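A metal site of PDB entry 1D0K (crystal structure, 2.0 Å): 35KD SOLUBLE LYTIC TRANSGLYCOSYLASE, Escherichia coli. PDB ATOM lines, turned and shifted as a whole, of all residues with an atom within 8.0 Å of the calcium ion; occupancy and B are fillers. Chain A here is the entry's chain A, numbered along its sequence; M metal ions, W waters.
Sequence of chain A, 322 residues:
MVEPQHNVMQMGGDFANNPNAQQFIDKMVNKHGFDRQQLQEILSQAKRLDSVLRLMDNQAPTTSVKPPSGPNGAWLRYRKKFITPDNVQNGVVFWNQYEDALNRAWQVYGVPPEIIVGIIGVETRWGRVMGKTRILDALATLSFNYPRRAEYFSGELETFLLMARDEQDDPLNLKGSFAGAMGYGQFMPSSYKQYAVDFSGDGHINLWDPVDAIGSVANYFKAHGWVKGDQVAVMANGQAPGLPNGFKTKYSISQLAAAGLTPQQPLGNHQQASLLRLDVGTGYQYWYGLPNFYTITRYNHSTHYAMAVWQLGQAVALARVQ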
ATOM      1  N   GLU A 167     -13.482  22.194  31.836  1.00  0.00           N
ATOM      2  CA  GLU A 167     -14.509  21.752  30.897  1.00  0.00           C
ATOM      3  C   GLU A 167     -14.485  20.225  30.739  1.00  0.00           C
ATOM      4  O   GLU A 167     -15.124  19.681  29.838  1.00  0.00           O
ATOM      5  CB  GLU A 167     -14.333  22.404  29.526  1.00  0.00           C
ATOM      6  CG  GLU A 167     -14.487  23.928  29.505  1.00  0.00           C
ATOM      7  CD  GLU A 167     -15.902  24.418  29.818  1.00  0.00           C
ATOM      8  OE1 GLU A 167     -16.842  23.601  29.875  1.00  0.00           O
ATOM      9  OE2 GLU A 167     -16.070  25.637  29.997  1.00  0.00           O
ATOM     10  N   VAL A 197     -17.970  32.849  26.234  1.00  0.00           N
ATOM     11  CA  VAL A 197     -19.184  32.769  27.043  1.00  0.00           C
ATOM     12  C   VAL A 197     -20.041  31.574  26.649  1.00  0.00           C
ATOM     13  O   VAL A 197     -19.958  31.074  25.519  1.00  0.00           O
ATOM     14  CB  VAL A 197     -20.054  34.060  26.947  1.00  0.00           C
ATOM     15  CG1 VAL A 197     -19.308  35.266  27.508  1.00  0.00           C
ATOM     16  CG2 VAL A 197     -20.473  34.315  25.505  1.00  0.00           C
ATOM     17  N   ASP A 198     -20.805  31.078  27.606  1.00  0.00           N
ATOM     18  CA  ASP A 198     -21.706  29.966  27.370  1.00  0.00           C
ATOM     19  C   ASP A 198     -22.982  30.578  26.798  1.00  0.00           C
ATOM     20  O   ASP A 198     -23.972  30.740  27.508  1.00  0.00           O
ATOM     21  CB  ASP A 198     -21.990  29.217  28.678  1.00  0.00           C
ATOM     22  CG  ASP A 198     -23.118  28.223  28.557  1.00  0.00           C
ATOM     23  OD1 ASP A 198     -23.292  27.643  27.464  1.00  0.00           O
ATOM     24  OD2 ASP A 198     -23.845  28.024  29.548  1.00  0.00           O
ATOM     25  N   PHE A 199     -22.950  30.942  25.525  1.00  0.00           N
ATOM     26  CA  PHE A 199     -24.093  31.568  24.881  1.00  0.00           C
ATOM     27  C   PHE A 199     -25.260  30.599  24.602  1.00  0.00           C
ATOM     28  O   PHE A 199     -26.402  31.049  24.441  1.00  0.00           O
ATOM     29  CB  PHE A 199     -23.664  32.272  23.586  1.00  0.00           C
ATOM     30  CG  PHE A 199     -24.487  33.501  23.256  1.00  0.00           C
ATOM     31  CD1 PHE A 199     -24.669  34.495  24.214  1.00  0.00           C
ATOM     32  CD2 PHE A 199     -25.036  33.664  21.991  1.00  0.00           C
ATOM     33  CE1 PHE A 199     -25.399  35.651  23.907  1.00  0.00           C
ATOM     34  CE2 PHE A 199     -25.774  34.818  21.678  1.00  0.00           C
ATOM     35  CZ  PHE A 199     -25.948  35.814  22.641  1.00  0.00           C
ATOM     36  N   SER A 200     -24.970  29.305  24.557  1.00  0.00           N
ATOM     37  CA  SER A 200     -26.017  28.301  24.321  1.00  0.00           C
ATOM     38  C   SER A 200     -26.814  28.031  25.587  1.00  0.00           C
ATOM     39  O   SER A 200     -27.920  27.498  25.529  1.00  0.00           O
ATOM     40  CB  SER A 200     -25.419  27.000  23.780  1.00  0.00           C
ATOM     41  OG  SER A 200     -24.780  26.263  24.813  1.00  0.00           O
ATOM     42  N   GLY A 201     -26.209  28.344  26.738  1.00  0.00           N
ATOM     43  CA  GLY A 201     -26.861  28.172  28.019  1.00  0.00           C
ATOM     44  C   GLY A 201     -26.915  26.798  28.644  1.00  0.00           C
ATOM     45  O   GLY A 201     -27.715  26.574  29.538  1.00  0.00           O
ATOM     46  N   ASP A 202     -26.075  25.866  28.199  1.00  0.00           N
ATOM     47  CA  ASP A 202     -26.075  24.514  28.765  1.00  0.00           C
ATOM     48  C   ASP A 202     -25.108  24.372  29.942  1.00  0.00           C
ATOM     49  O   ASP A 202     -24.887  23.264  30.445  1.00  0.00           O
ATOM     50  CB  ASP A 202     -25.749  23.470  27.692  1.00  0.00           C
ATOM     51  CG  ASP A 202     -24.336  23.595  27.144  1.00  0.00           C
ATOM     52  OD1 ASP A 202     -23.715  24.652  27.323  1.00  0.00           O
ATOM     53  OD2 ASP A 202     -23.835  22.610  26.569  1.00  0.00           O
ATOM     54  N   GLY A 203     -24.517  25.494  30.366  1.00  0.00           N
ATOM     55  CA  GLY A 203     -23.580  25.491  31.469  1.00  0.00           C
ATOM     56  C   GLY A 203     -22.128  25.225  31.100  1.00  0.00           C
ATOM     57  O   GLY A 203     -21.251  25.274  31.965  1.00  0.00           O
ATOM     58  N   HIS A 204     -21.860  24.954  29.826  1.00  0.00           N
ATOM     59  CA  HIS A 204     -20.503  24.671  29.368  1.00  0.00           C
ATOM     60  C   HIS A 204     -20.049  25.583  28.235  1.00  0.00           C
ATOM     61  O   HIS A 204     -20.832  25.936  27.362  1.00  0.00           O
ATOM     62  CB  HIS A 204     -20.411  23.211  28.907  1.00  0.00           C
ATOM     63  CG  HIS A 204     -20.662  22.216  29.995  1.00  0.00           C
ATOM     64  ND1 HIS A 204     -19.642  21.537  30.630  1.00  0.00           N
ATOM     65  CD2 HIS A 204     -21.816  21.768  30.540  1.00  0.00           C
ATOM     66  CE1 HIS A 204     -20.168  20.718  31.528  1.00  0.00           C
ATOM     67  NE2 HIS A 204     -21.481  20.837  31.495  1.00  0.00           N
ATOM     68  N   ILE A 205     -18.798  26.018  28.292  1.00  0.00           N
ATOM     69  CA  ILE A 205     -18.261  26.872  27.238  1.00  0.00           C
ATOM     70  C   ILE A 205     -17.516  25.953  26.270  1.00  0.00           C
ATOM     71  O   ILE A 205     -16.473  25.394  26.592  1.00  0.00           O
ATOM     72  CB  ILE A 205     -17.328  27.975  27.780  1.00  0.00           C
ATOM     73  CG1 ILE A 205     -18.115  28.903  28.715  1.00  0.00           C
ATOM     74  CG2 ILE A 205     -16.774  28.820  26.624  1.00  0.00           C
ATOM     75  CD1 ILE A 205     -17.252  29.889  29.482  1.00  0.00           C
ATOM     76  N   ASN A 206     -18.107  25.762  25.093  1.00  0.00           N
ATOM     77  CA  ASN A 206     -17.538  24.907  24.063  1.00  0.00           C
ATOM     78  C   ASN A 206     -17.247  25.770  22.838  1.00  0.00           C
ATOM     79  O   ASN A 206     -18.161  26.272  22.195  1.00  0.00           O
ATOM     80  CB  ASN A 206     -18.537  23.798  23.736  1.00  0.00           C
ATOM     81  CG  ASN A 206     -18.039  22.843  22.647  1.00  0.00           C
ATOM     82  OD1 ASN A 206     -16.931  22.973  22.151  1.00  0.00           O
ATOM     83  ND2 ASN A 206     -18.886  21.889  22.291  1.00  0.00           N
ATOM     84  N   LEU A 207     -15.967  25.909  22.517  1.00  0.00           N
ATOM     85  CA  LEU A 207     -15.541  26.713  21.373  1.00  0.00           C
ATOM     86  C   LEU A 207     -15.954  26.083  20.038  1.00  0.00           C
ATOM     87  O   LEU A 207     -15.926  26.749  18.997  1.00  0.00           O
ATOM     88  CB  LEU A 207     -14.025  26.917  21.420  1.00  0.00           C
ATOM     89  CG  LEU A 207     -13.527  27.661  22.659  1.00  0.00           C
ATOM     90  CD1 LEU A 207     -12.007  27.689  22.680  1.00  0.00           C
ATOM     91  CD2 LEU A 207     -14.093  29.077  22.665  1.00  0.00           C
ATOM     92  N   ASP A 209     -18.983  24.766  19.588  1.00  0.00           N
ATOM     93  CA  ASP A 209     -20.439  24.885  19.504  1.00  0.00           C
ATOM     94  C   ASP A 209     -20.619  26.244  18.833  1.00  0.00           C
ATOM     95  O   ASP A 209     -20.206  27.270  19.382  1.00  0.00           O
ATOM     96  CB  ASP A 209     -21.054  24.909  20.919  1.00  0.00           C
ATOM     97  CG  ASP A 209     -22.591  25.014  20.925  1.00  0.00           C
ATOM     98  OD1 ASP A 209     -23.186  25.622  20.026  1.00  0.00           O
ATOM     99  OD2 ASP A 209     -23.222  24.489  21.872  1.00  0.00           O
ATOM    100  N   VAL A 211     -23.112  28.225  18.541  1.00  0.00           N
ATOM    101  CA  VAL A 211     -23.862  29.185  19.353  1.00  0.00           C
ATOM    102  C   VAL A 211     -22.943  29.861  20.351  1.00  0.00           C
ATOM    103  O   VAL A 211     -22.960  31.090  20.484  1.00  0.00           O
ATOM    104  CB  VAL A 211     -25.078  28.531  20.062  1.00  0.00           C
ATOM    105  CG1 VAL A 211     -25.745  29.532  21.004  1.00  0.00           C
ATOM    106  CG2 VAL A 211     -26.084  28.061  19.024  1.00  0.00           C
ATOM    107  N   ASP A 212     -22.114  29.075  21.049  1.00  0.00           N
ATOM    108  CA  ASP A 212     -21.164  29.619  22.018  1.00  0.00           C
ATOM    109  C   ASP A 212     -20.137  30.518  21.316  1.00  0.00           C
ATOM    110  O   ASP A 212     -19.752  31.566  21.843  1.00  0.00           O
ATOM    111  CB  ASP A 212     -20.397  28.497  22.726  1.00  0.00           C
ATOM    112  CG  ASP A 212     -21.185  27.875  23.853  1.00  0.00           C
ATOM    113  OD1 ASP A 212     -22.424  28.048  23.905  1.00  0.00           O
ATOM    114  OD2 ASP A 212     -20.558  27.206  24.699  1.00  0.00           O
ATOM    115  N   ALA A 213     -19.684  30.067  20.149  1.00  0.00           N
ATOM    116  CA  ALA A 213     -18.692  30.806  19.365  1.00  0.00           C
ATOM    117  C   ALA A 213     -19.237  32.163  18.939  1.00  0.00           C
ATOM    118  O   ALA A 213     -18.528  33.160  18.996  1.00  0.00           O
ATOM    119  CB  ALA A 213     -18.292  30.001  18.137  1.00  0.00           C
HETATM  120 CA    CA M   1     -22.552  26.123  25.754  1.00  0.00          CA
HETATM  121  O   HOH W   1     -22.305  24.255  24.221  1.00  0.00           O
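N of Gly 203 sits at hydrogen-bond distance from OD2 of Asp 198, at 2.7 Å. N of Gly 201 lies close to OD1 of Asp 198, 3.1 Å away. The side-chain carboxylate (OD2) of Asp 212 sits close to the backbone NH (N) of Asn 206 (2.9 Å). The side-chain carboxylate of Asp 212 lies close to the backbone NH of Phe 199.
Within 4 Å of the calcium ion: Asp 198, Ser 200, Asp 202, His 204 and Asp 212. Along chain A the residues within 4 Å of the calcium ion span positions 198 to 212.
The calcium ion is bound by the backbone carbonyl oxygen (O) of His 204 (2.4 Å), the side-chain carboxylate (OD1) of Asp 198 (2.4 Å), the side-chain hydroxyl (OG) of Ser 200 (2.4 Å), water W1 (2.4 Å), the side-chain carboxylate (OD1) of Asp 202 (2.4 Å), the side-chain carboxylate (OD2) of Asp 212 (2.5 Å) and the side-chain carboxylate (OD1) of Asp 212 (2.7 Å). The calcium ion has seven donor atoms within binding distance.
Water W1 lies within hydrogen-bond range of OD2 of Asp 209 (2.5 Å) and OD2 of Asp 202 (3.2 Å).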
